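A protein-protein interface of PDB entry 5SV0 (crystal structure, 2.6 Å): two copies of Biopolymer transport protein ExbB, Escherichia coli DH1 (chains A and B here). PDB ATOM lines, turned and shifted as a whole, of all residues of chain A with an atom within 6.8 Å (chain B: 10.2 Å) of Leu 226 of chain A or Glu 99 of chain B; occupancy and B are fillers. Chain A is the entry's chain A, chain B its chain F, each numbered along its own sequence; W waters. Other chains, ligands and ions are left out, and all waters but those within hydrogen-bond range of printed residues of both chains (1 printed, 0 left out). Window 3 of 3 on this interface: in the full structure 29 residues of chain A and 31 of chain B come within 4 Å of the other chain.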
ATOM      1  N   SER A 221      -9.012  18.926  14.952  1.00  0.00           N
ATOM      2  CA  SER A 221      -8.106  18.549  13.857  1.00  0.00           C
ATOM      3  C   SER A 221      -8.191  19.531  12.688  1.00  0.00           C
ATOM      4  O   SER A 221      -7.171  20.085  12.243  1.00  0.00           O
ATOM      5  CB  SER A 221      -8.423  17.115  13.391  1.00  0.00           C
ATOM      6  OG  SER A 221      -7.570  16.647  12.341  1.00  0.00           O
ATOM      7  N   ARG A 222      -9.409  19.780  12.198  1.00  0.00           N
ATOM      8  CA  ARG A 222      -9.582  20.694  11.071  1.00  0.00           C
ATOM      9  C   ARG A 222      -9.076  22.089  11.402  1.00  0.00           C
ATOM     10  O   ARG A 222      -8.397  22.717  10.581  1.00  0.00           O
ATOM     11  CB  ARG A 222     -11.063  20.753  10.681  1.00  0.00           C
ATOM     12  CG  ARG A 222     -11.423  20.957   9.182  1.00  0.00           C
ATOM     13  CD  ARG A 222     -12.653  20.029   8.801  1.00  0.00           C
ATOM     14  NE  ARG A 222     -13.728  20.085   9.799  1.00  0.00           N
ATOM     15  CZ  ARG A 222     -14.576  19.097  10.072  1.00  0.00           C
ATOM     16  NH1 ARG A 222     -14.496  17.943   9.430  1.00  0.00           N
ATOM     17  NH2 ARG A 222     -15.499  19.257  11.011  1.00  0.00           N
ATOM     18  N   ASP A 223      -9.395  22.593  12.601  1.00  0.00           N
ATOM     19  CA  ASP A 223      -8.981  23.938  12.983  1.00  0.00           C
ATOM     20  C   ASP A 223      -7.465  24.055  13.105  1.00  0.00           C
ATOM     21  O   ASP A 223      -6.870  25.029  12.620  1.00  0.00           O
ATOM     22  CB  ASP A 223      -9.717  24.347  14.244  1.00  0.00           C
ATOM     23  CG  ASP A 223     -11.202  24.639  13.967  1.00  0.00           C
ATOM     24  OD1 ASP A 223     -11.750  24.122  12.963  1.00  0.00           O
ATOM     25  OD2 ASP A 223     -11.823  25.408  14.738  1.00  0.00           O
ATOM     26  N   LEU A 224      -6.815  23.074  13.726  1.00  0.00           N
ATOM     27  CA  LEU A 224      -5.360  23.109  13.761  1.00  0.00           C
ATOM     28  C   LEU A 224      -4.791  23.169  12.352  1.00  0.00           C
ATOM     29  O   LEU A 224      -3.858  23.933  12.087  1.00  0.00           O
ATOM     30  CB  LEU A 224      -4.809  21.886  14.492  1.00  0.00           C
ATOM     31  CG  LEU A 224      -5.016  21.889  15.998  1.00  0.00           C
ATOM     32  CD1 LEU A 224      -4.622  20.570  16.625  1.00  0.00           C
ATOM     33  CD2 LEU A 224      -4.297  23.045  16.607  1.00  0.00           C
ATOM     34  N   ASP A 225      -5.329  22.359  11.431  1.00  0.00           N
ATOM     35  CA  ASP A 225      -4.759  22.356  10.086  1.00  0.00           C
ATOM     36  C   ASP A 225      -5.044  23.664   9.365  1.00  0.00           C
ATOM     37  O   ASP A 225      -4.186  24.184   8.658  1.00  0.00           O
ATOM     38  CB  ASP A 225      -5.264  21.158   9.276  1.00  0.00           C
ATOM     39  CG  ASP A 225      -4.790  19.848   9.868  1.00  0.00           C
ATOM     40  OD1 ASP A 225      -4.252  19.876  10.994  1.00  0.00           O
ATOM     41  OD2 ASP A 225      -4.908  18.801   9.223  1.00  0.00           O
ATOM     42  N   LEU A 226      -6.236  24.221   9.521  1.00  0.00           N
ATOM     43  CA  LEU A 226      -6.513  25.459   8.806  1.00  0.00           C
ATOM     44  C   LEU A 226      -5.651  26.591   9.338  1.00  0.00           C
ATOM     45  O   LEU A 226      -5.162  27.422   8.568  1.00  0.00           O
ATOM     46  CB  LEU A 226      -8.005  25.786   8.880  1.00  0.00           C
ATOM     47  CG  LEU A 226      -8.885  24.839   8.032  1.00  0.00           C
ATOM     48  CD1 LEU A 226     -10.348  25.052   8.324  1.00  0.00           C
ATOM     49  CD2 LEU A 226      -8.644  25.082   6.552  1.00  0.00           C
ATOM     50  N   GLU A 227      -5.433  26.624  10.647  1.00  0.00           N
ATOM     51  CA  GLU A 227      -4.536  27.610  11.239  1.00  0.00           C
ATOM     52  C   GLU A 227      -3.107  27.427  10.744  1.00  0.00           C
ATOM     53  O   GLU A 227      -2.409  28.405  10.450  1.00  0.00           O
ATOM     54  CB  GLU A 227      -4.609  27.489  12.754  1.00  0.00           C
ATOM     55  CG  GLU A 227      -3.754  28.408  13.523  1.00  0.00           C
ATOM     56  CD  GLU A 227      -3.796  28.072  14.993  1.00  0.00           C
ATOM     57  OE1 GLU A 227      -3.443  26.918  15.343  1.00  0.00           O
ATOM     58  OE2 GLU A 227      -4.188  28.957  15.793  1.00  0.00           O
ATOM     59  N   ALA A 228      -2.639  26.181  10.680  1.00  0.00           N
ATOM     60  CA  ALA A 228      -1.286  25.936  10.193  1.00  0.00           C
ATOM     61  C   ALA A 228      -1.140  26.377   8.745  1.00  0.00           C
ATOM     62  O   ALA A 228      -0.100  26.919   8.358  1.00  0.00           O
ATOM     63  CB  ALA A 228      -0.933  24.459  10.348  1.00  0.00           C
ATOM     64  N   SER A 229      -2.172  26.149   7.929  1.00  0.00           N
ATOM     65  CA  SER A 229      -2.113  26.525   6.516  1.00  0.00           C
ATOM     66  C   SER A 229      -2.203  28.038   6.335  1.00  0.00           C
ATOM     67  O   SER A 229      -1.601  28.598   5.413  1.00  0.00           O
ATOM     68  CB  SER A 229      -3.225  25.816   5.755  1.00  0.00           C
ATOM     69  OG  SER A 229      -3.140  24.411   5.966  1.00  0.00           O
ATOM     70  N   ALA A 230      -3.002  28.707   7.162  1.00  0.00           N
ATOM     71  CA  ALA A 230      -3.093  30.158   7.074  1.00  0.00           C
ATOM     72  C   ALA A 230      -1.828  30.816   7.578  1.00  0.00           C
ATOM     73  O   ALA A 230      -1.479  31.909   7.124  1.00  0.00           O
ATOM     74  CB  ALA A 230      -4.300  30.672   7.863  1.00  0.00           C
ATOM     75  N   ALA A 231      -1.106  30.154   8.483  1.00  0.00           N
ATOM     76  CA  ALA A 231       0.151  30.714   8.957  1.00  0.00           C
ATOM     77  C   ALA A 231       1.264  30.538   7.941  1.00  0.00           C
ATOM     78  O   ALA A 231       2.152  31.389   7.848  1.00  0.00           O
ATOM     79  CB  ALA A 231       0.551  30.071  10.284  1.00  0.00           C
ATOM     80  N   ALA B  91     -18.036  12.506   2.099  1.00  0.00           N
ATOM     81  CA  ALA B  91     -16.648  12.727   1.701  1.00  0.00           C
ATOM     82  C   ALA B  91     -16.464  14.091   1.040  1.00  0.00           C
ATOM     83  O   ALA B  91     -15.481  14.806   1.306  1.00  0.00           O
ATOM     84  CB  ALA B  91     -16.198  11.593   0.782  1.00  0.00           C
ATOM     85  N   GLN B  92     -17.395  14.474   0.167  1.00  0.00           N
ATOM     86  CA  GLN B  92     -17.332  15.810  -0.413  1.00  0.00           C
ATOM     87  C   GLN B  92     -17.416  16.882   0.674  1.00  0.00           C
ATOM     88  O   GLN B  92     -16.771  17.939   0.586  1.00  0.00           O
ATOM     89  CB  GLN B  92     -18.450  15.992  -1.439  1.00  0.00           C
ATOM     90  CG  GLN B  92     -18.381  17.323  -2.148  1.00  0.00           C
ATOM     91  CD  GLN B  92     -17.087  17.503  -2.884  1.00  0.00           C
ATOM     92  OE1 GLN B  92     -16.496  16.538  -3.382  1.00  0.00           O
ATOM     93  NE2 GLN B  92     -16.604  18.733  -2.916  1.00  0.00           N
ATOM     94  N   ASN B  93     -18.223  16.631   1.701  1.00  0.00           N
ATOM     95  CA  ASN B  93     -18.370  17.618   2.760  1.00  0.00           C
ATOM     96  C   ASN B  93     -17.053  17.818   3.493  1.00  0.00           C
ATOM     97  O   ASN B  93     -16.682  18.956   3.821  1.00  0.00           O
ATOM     98  CB  ASN B  93     -19.516  17.208   3.704  1.00  0.00           C
ATOM     99  CG  ASN B  93     -19.774  18.237   4.771  1.00  0.00           C
ATOM    100  OD1 ASN B  93     -19.586  17.982   5.963  1.00  0.00           O
ATOM    101  ND2 ASN B  93     -20.108  19.450   4.339  1.00  0.00           N
ATOM    102  N   GLU B  94     -16.315  16.729   3.727  1.00  0.00           N
ATOM    103  CA  GLU B  94     -15.006  16.880   4.355  1.00  0.00           C
ATOM    104  C   GLU B  94     -14.074  17.697   3.480  1.00  0.00           C
ATOM    105  O   GLU B  94     -13.347  18.558   3.988  1.00  0.00           O
ATOM    106  CB  GLU B  94     -14.359  15.541   4.661  1.00  0.00           C
ATOM    107  CG  GLU B  94     -13.135  15.721   5.552  1.00  0.00           C
ATOM    108  CD  GLU B  94     -13.400  16.504   6.853  1.00  0.00           C
ATOM    109  OE1 GLU B  94     -12.661  17.469   7.168  1.00  0.00           O
ATOM    110  OE2 GLU B  94     -14.332  16.121   7.594  1.00  0.00           O
ATOM    111  N   LEU B  95     -14.090  17.453   2.160  1.00  0.00           N
ATOM    112  CA  LEU B  95     -13.276  18.279   1.265  1.00  0.00           C
ATOM    113  C   LEU B  95     -13.640  19.762   1.375  1.00  0.00           C
ATOM    114  O   LEU B  95     -12.757  20.624   1.408  1.00  0.00           O
ATOM    115  CB  LEU B  95     -13.436  17.811  -0.174  1.00  0.00           C
ATOM    116  CG  LEU B  95     -12.805  16.461  -0.451  1.00  0.00           C
ATOM    117  CD1 LEU B  95     -13.223  15.980  -1.844  1.00  0.00           C
ATOM    118  CD2 LEU B  95     -11.311  16.564  -0.297  1.00  0.00           C
ATOM    119  N   GLU B  96     -14.938  20.085   1.410  1.00  0.00           N
ATOM    120  CA  GLU B  96     -15.330  21.489   1.432  1.00  0.00           C
ATOM    121  C   GLU B  96     -14.964  22.155   2.757  1.00  0.00           C
ATOM    122  O   GLU B  96     -14.581  23.333   2.776  1.00  0.00           O
ATOM    123  CB  GLU B  96     -16.824  21.638   1.143  1.00  0.00           C
ATOM    124  CG  GLU B  96     -17.271  21.247  -0.264  1.00  0.00           C
ATOM    125  CD  GLU B  96     -18.816  21.203  -0.417  1.00  0.00           C
ATOM    126  OE1 GLU B  96     -19.551  21.740   0.460  1.00  0.00           O
ATOM    127  OE2 GLU B  96     -19.297  20.611  -1.416  1.00  0.00           O
ATOM    128  N   LEU B  97     -15.116  21.440   3.884  1.00  0.00           N
ATOM    129  CA  LEU B  97     -14.763  22.035   5.174  1.00  0.00           C
ATOM    130  C   LEU B  97     -13.263  22.253   5.339  1.00  0.00           C
ATOM    131  O   LEU B  97     -12.852  23.179   6.042  1.00  0.00           O
ATOM    132  CB  LEU B  97     -15.282  21.169   6.320  1.00  0.00           C
ATOM    133  CG  LEU B  97     -16.767  21.221   6.651  1.00  0.00           C
ATOM    134  CD1 LEU B  97     -17.101  20.210   7.727  1.00  0.00           C
ATOM    135  CD2 LEU B  97     -17.040  22.613   7.157  1.00  0.00           C
ATOM    136  N   SER B  98     -12.439  21.428   4.707  1.00  0.00           N
ATOM    137  CA  SER B  98     -11.000  21.533   4.812  1.00  0.00           C
ATOM    138  C   SER B  98     -10.416  22.392   3.719  1.00  0.00           C
ATOM    139  O   SER B  98      -9.190  22.496   3.633  1.00  0.00           O
ATOM    140  CB  SER B  98     -10.356  20.162   4.711  1.00  0.00           C
ATOM    141  OG  SER B  98     -10.787  19.314   5.738  1.00  0.00           O
ATOM    142  N   GLU B  99     -11.258  22.951   2.851  1.00  0.00           N
ATOM    143  CA  GLU B  99     -10.787  23.845   1.806  1.00  0.00           C
ATOM    144  C   GLU B  99      -9.900  24.898   2.442  1.00  0.00           C
ATOM    145  O   GLU B  99     -10.248  25.470   3.478  1.00  0.00           O
ATOM    146  CB  GLU B  99     -11.976  24.497   1.088  1.00  0.00           C
ATOM    147  CG  GLU B  99     -11.694  25.072  -0.296  1.00  0.00           C
ATOM    148  CD  GLU B  99     -11.445  23.996  -1.363  1.00  0.00           C
ATOM    149  OE1 GLU B  99     -11.728  22.793  -1.130  1.00  0.00           O
ATOM    150  OE2 GLU B  99     -10.951  24.356  -2.449  1.00  0.00           O
ATOM    151  N   GLY B 100      -8.728  25.102   1.858  1.00  0.00           N
ATOM    152  CA  GLY B 100      -7.759  26.019   2.399  1.00  0.00           C
ATOM    153  C   GLY B 100      -6.715  25.373   3.274  1.00  0.00           C
ATOM    154  O   GLY B 100      -5.755  26.046   3.661  1.00  0.00           O
ATOM    155  N   SER B 101      -6.868  24.098   3.607  1.00  0.00           N
ATOM    156  CA  SER B 101      -5.866  23.394   4.385  1.00  0.00           C
ATOM    157  C   SER B 101      -4.871  22.720   3.456  1.00  0.00           C
ATOM    158  O   SER B 101      -5.259  22.058   2.491  1.00  0.00           O
ATOM    159  CB  SER B 101      -6.499  22.344   5.283  1.00  0.00           C
ATOM    160  OG  SER B 101      -5.488  21.551   5.860  1.00  0.00           O
ATOM    161  N   ASP B 102      -3.591  22.832   3.805  1.00  0.00           N
ATOM    162  CA  ASP B 102      -2.478  22.220   3.097  1.00  0.00           C
ATOM    163  C   ASP B 102      -2.238  20.769   3.483  1.00  0.00           C
ATOM    164  O   ASP B 102      -1.447  20.097   2.814  1.00  0.00           O
ATOM    165  CB  ASP B 102      -1.204  23.011   3.381  1.00  0.00           C
ATOM    166  CG  ASP B 102      -1.303  24.446   2.922  1.00  0.00           C
ATOM    167  OD1 ASP B 102      -2.084  24.712   1.976  1.00  0.00           O
ATOM    168  OD2 ASP B 102      -0.622  25.308   3.530  1.00  0.00           O
ATOM    169  N   ASP B 103      -2.884  20.263   4.532  1.00  0.00           N
ATOM    170  CA  ASP B 103      -2.548  18.963   5.099  1.00  0.00           C
ATOM    171  C   ASP B 103      -3.539  17.919   4.584  1.00  0.00           C
ATOM    172  O   ASP B 103      -4.653  17.778   5.101  1.00  0.00           O
ATOM    173  CB  ASP B 103      -2.550  19.062   6.620  1.00  0.00           C
ATOM    174  CG  ASP B 103      -2.077  17.799   7.288  1.00  0.00           C
ATOM    175  OD1 ASP B 103      -1.946  16.785   6.579  1.00  0.00           O
ATOM    176  OD2 ASP B 103      -1.821  17.810   8.514  1.00  0.00           O
ATOM    177  N   ASN B 104      -3.080  17.101   3.632  1.00  0.00           N
ATOM    178  CA  ASN B 104      -3.948  16.069   3.093  1.00  0.00           C
ATOM    179  C   ASN B 104      -4.038  14.858   4.002  1.00  0.00           C
ATOM    180  O   ASN B 104      -5.067  14.172   3.974  1.00  0.00           O
ATOM    181  CB  ASN B 104      -3.504  15.681   1.696  1.00  0.00           C
ATOM    182  CG  ASN B 104      -3.808  16.762   0.672  1.00  0.00           C
ATOM    183  OD1 ASN B 104      -4.518  17.735   0.956  1.00  0.00           O
ATOM    184  ND2 ASN B 104      -3.305  16.576  -0.539  1.00  0.00           N
ATOM    185  N   GLY B 106      -4.519  15.043   7.165  1.00  0.00           N
ATOM    186  CA  GLY B 106      -5.662  15.365   8.001  1.00  0.00           C
ATOM    187  C   GLY B 106      -6.982  15.067   7.319  1.00  0.00           C
ATOM    188  O   GLY B 106      -7.804  14.320   7.844  1.00  0.00           O
ATOM    189  N   ILE B 107      -7.126  15.512   6.089  1.00  0.00           N
ATOM    190  CA  ILE B 107      -8.337  15.308   5.315  1.00  0.00           C
ATOM    191  C   ILE B 107      -8.664  13.812   5.256  1.00  0.00           C
ATOM    192  O   ILE B 107      -9.733  13.392   5.742  1.00  0.00           O
ATOM    193  CB  ILE B 107      -8.182  15.904   3.919  1.00  0.00           C
ATOM    194  CG1 ILE B 107      -7.898  17.401   4.012  1.00  0.00           C
ATOM    195  CG2 ILE B 107      -9.448  15.726   3.137  1.00  0.00           C
ATOM    196  CD1 ILE B 107      -7.569  18.049   2.695  1.00  0.00           C
ATOM    197  N   ARG B 110      -9.675  12.482   8.713  1.00  0.00           N
ATOM    198  CA  ARG B 110     -11.005  12.922   9.099  1.00  0.00           C
ATOM    199  C   ARG B 110     -12.063  12.189   8.294  1.00  0.00           C
ATOM    200  O   ARG B 110     -13.123  11.822   8.824  1.00  0.00           O
ATOM    201  CB  ARG B 110     -11.139  14.429   8.883  1.00  0.00           C
ATOM    202  CG  ARG B 110     -10.628  15.259   9.998  1.00  0.00           C
ATOM    203  CD  ARG B 110     -10.826  16.769   9.731  1.00  0.00           C
ATOM    204  NE  ARG B 110      -9.529  17.337   9.913  1.00  0.00           N
ATOM    205  CZ  ARG B 110      -8.774  17.875   8.982  1.00  0.00           C
ATOM    206  NH1 ARG B 110      -9.214  18.024   7.748  1.00  0.00           N
ATOM    207  NH2 ARG B 110      -7.562  18.273   9.336  1.00  0.00           N
ATOM    208  N   ARG B 114     -15.003   9.586   9.663  1.00  0.00           N
ATOM    209  CA  ARG B 114     -16.424   9.865   9.510  1.00  0.00           C
ATOM    210  C   ARG B 114     -17.148   8.679   8.896  1.00  0.00           C
ATOM    211  O   ARG B 114     -18.159   8.204   9.454  1.00  0.00           O
ATOM    212  CB  ARG B 114     -16.642  11.147   8.711  1.00  0.00           C
ATOM    213  CG  ARG B 114     -16.417  12.430   9.552  1.00  0.00           C
ATOM    214  CD  ARG B 114     -16.481  13.693   8.666  1.00  0.00           C
ATOM    215  NE  ARG B 114     -17.830  14.132   8.355  1.00  0.00           N
ATOM    216  CZ  ARG B 114     -18.121  15.145   7.553  1.00  0.00           C
ATOM    217  NH1 ARG B 114     -17.148  15.818   6.956  1.00  0.00           N
ATOM    218  NH2 ARG B 114     -19.389  15.467   7.326  1.00  0.00           N
ATOM    219  N   GLN B 220     -10.914   9.207  -2.929  1.00  0.00           N
ATOM    220  CA  GLN B 220     -10.489  10.481  -2.341  1.00  0.00           C
ATOM    221  C   GLN B 220      -8.969  10.553  -2.118  1.00  0.00           C
ATOM    222  O   GLN B 220      -8.322  11.558  -2.431  1.00  0.00           O
ATOM    223  CB  GLN B 220     -11.215  10.700  -1.033  1.00  0.00           C
ATOM    224  CG  GLN B 220     -10.985  12.080  -0.544  1.00  0.00           C
ATOM    225  CD  GLN B 220     -11.266  12.188   0.899  1.00  0.00           C
ATOM    226  OE1 GLN B 220     -10.773  11.379   1.708  1.00  0.00           O
ATOM    227  NE2 GLN B 220     -12.102  13.171   1.256  1.00  0.00           N
ATOM    228  N   LEU B 224      -6.452  13.258  -3.965  1.00  0.00           N
ATOM    229  CA  LEU B 224      -5.621  14.203  -3.224  1.00  0.00           C
ATOM    230  C   LEU B 224      -4.144  14.078  -3.613  1.00  0.00           C
ATOM    231  O   LEU B 224      -3.468  15.081  -3.891  1.00  0.00           O
ATOM    232  CB  LEU B 224      -5.815  13.999  -1.723  1.00  0.00           C
ATOM    233  CG  LEU B 224      -7.139  14.528  -1.149  1.00  0.00           C
ATOM    234  CD1 LEU B 224      -7.350  14.013   0.273  1.00  0.00           C
ATOM    235  CD2 LEU B 224      -7.162  16.044  -1.163  1.00  0.00           C
ATOM    236  N   GLU B 227      -3.547  15.375  -7.281  1.00  0.00           N
ATOM    237  CA  GLU B 227      -3.582  16.841  -7.333  1.00  0.00           C
ATOM    238  C   GLU B 227      -2.316  17.441  -6.716  1.00  0.00           C
ATOM    239  O   GLU B 227      -1.741  18.407  -7.239  1.00  0.00           O
ATOM    240  CB  GLU B 227      -4.832  17.336  -6.625  1.00  0.00           C
ATOM    241  CG  GLU B 227      -6.096  16.978  -7.376  1.00  0.00           C
ATOM    242  CD  GLU B 227      -7.333  16.958  -6.485  1.00  0.00           C
ATOM    243  OE1 GLU B 227      -8.278  16.209  -6.810  1.00  0.00           O
ATOM    244  OE2 GLU B 227      -7.356  17.671  -5.454  1.00  0.00           O
HETATM  245  O   HOH W   1      -6.316  19.359   6.869  1.00  0.00           O
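Of the printed residues of chain B, Arg 222 of chain A touches Glu 94, Leu 97, Ser 98 and Arg 110.
Of chain B, only Ser 101, Asp 103, Gly 106 and Arg 110 come within 4 Å of Asp 225 of chain A.
Of chain B, only Leu 97 (3.9 Å), Ser 98 (3.9 Å), Glu 99 (3.5 Å), Gly 100 (3.8 Å) and Ser 101 (3.6 Å) come within 4 Å of Leu 226 of chain A.
No residue of chain B comes within 4 Å of Ala 228 of chain A.
Of chain B, only Gly 100, Ser 101 and Asp 102 come within 4 Å of Ser 229 of chain A.
No residue of chain B comes within 4 Å of Ala 230 of chain A.
Ala 231 of chain A touches none of the printed residues of chain B.
Of the printed residues of chain A, Ser 98 of chain B touches Arg 222 (3.7 Å) and Leu 226 (3.9 Å).
Of chain A, only Leu 226 (3.5 Å) comes within 4 Å of Glu 99 of chain B.
Of the printed residues of chain A, Gly 100 of chain B touches Leu 226 and Ser 229.
Of the printed residues of chain A, Gly 106 of chain B touches Asp 225.
The nearest residue of chain A that does not touch Glu 99 of chain B is Arg 222 of chain A (6.6 Å).
The nearest printed residue of chain A that does not touch Asp 102 of chain B is Asp 225 of chain A (5.1 Å).
The backbone NH (N) of Asp 103 of chain B lies within hydrogen-bond range of the side-chain hydroxyl (OG) of Ser 101 of chain B.
The side-chain carboxylate (OE1) of Glu 94 of chain B is in hydrogen-bond range of the side-chain hydroxyl (OG) of Ser 98 of chain B.
The guanidinium group (NH1) of Arg 110 of chain B lies within salt-bridge range of the side-chain carboxylate (OE1) of Glu 94 of chain B (3.5 Å).
The backbone carbonyl oxygen of Asp 225 of chain A sits at hydrogen-bond distance from the side-chain hydroxyl of Ser 229 of chain A, 2.9 Å away.
The side-chain carboxylate (OD1) of Asp 103 of chain B is in hydrogen-bond range of the backbone NH (N) of Gly 106 of chain B, 3.2 Å away.
OG of Ser 98 of chain B sits at hydrogen-bond distance from NH1 of Arg 110 of chain B (2.9 Å).
N of Asp 102 of chain B lies within hydrogen-bond range of OG of Ser 229 of chain A, 2.7 Å away.
The guanidinium group of Arg 110 of chain B sits close to the backbone NH of Arg 222 of chain A, 3.3 Å away.
NH2 of Arg 110 of chain B lies within salt-bridge range of OD2 of Asp 225 of chain A, at 2.7 Å.
NH1 of Arg 222 of chain A is in salt-bridge range of OE2 of Glu 94 of chain B.
OD2 of Asp 225 of chain A sits close to OD2 of Asp 103 of chain B (3.3 Å).
NE of Arg 110 of chain B sits at hydrogen-bond distance from OG of Ser 221 of chain A.
Hydrophobic or aromatic side chains of chain A within 4 Å of the printed part of chain B: Leu 226.
Hydrophobic or aromatic side chains of chain B within 4 Å of the printed part of chain A: Leu 97.
Among the printed residues, 17 pairs touch across the chains.
Among the printed residues, Asp or Glu carboxylates within 4 Å of a Lys or Arg side-chain nitrogen of the other chain: Arg 222 of chain A with Glu 94 of chain B (2.6 Å) and Asp 225 of chain A with Arg 110 of chain B (2.7 Å).
Water W1 lies within hydrogen-bond range of OG of Ser 101 of chain B, OD2 of Asp 225 of chain A, O of Asp 103 of chain B and NH2 of Arg 110 of chain B.
Among the printed residues, merely in contact across the chains: Arg 222 of chain A with Leu 97 of chain B, Arg 222 of chain A with Ser 98 of chain B, Asp 225 of chain A with Ser 101 of chain B, Asp 225 of chain A with Gly 106 of chain B, Leu 226 of chain A with Leu 97 of chain B, Leu 226 of chain A with Ser 98 of chain B, Leu 226 of chain A with Glu 99 of chain B, Leu 226 of chain A with Gly 100 of chain B, Leu 226 of chain A with Ser 101 of chain B, Ser 229 of chain A with Gly 100 of chain B and Ser 229 of chain A with Ser 101 of chain B.
2 positions are printed for both chains.
Of the 17 pairs that touch across the chains among the printed residues, none has its exchanged pair printed and touching as well.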
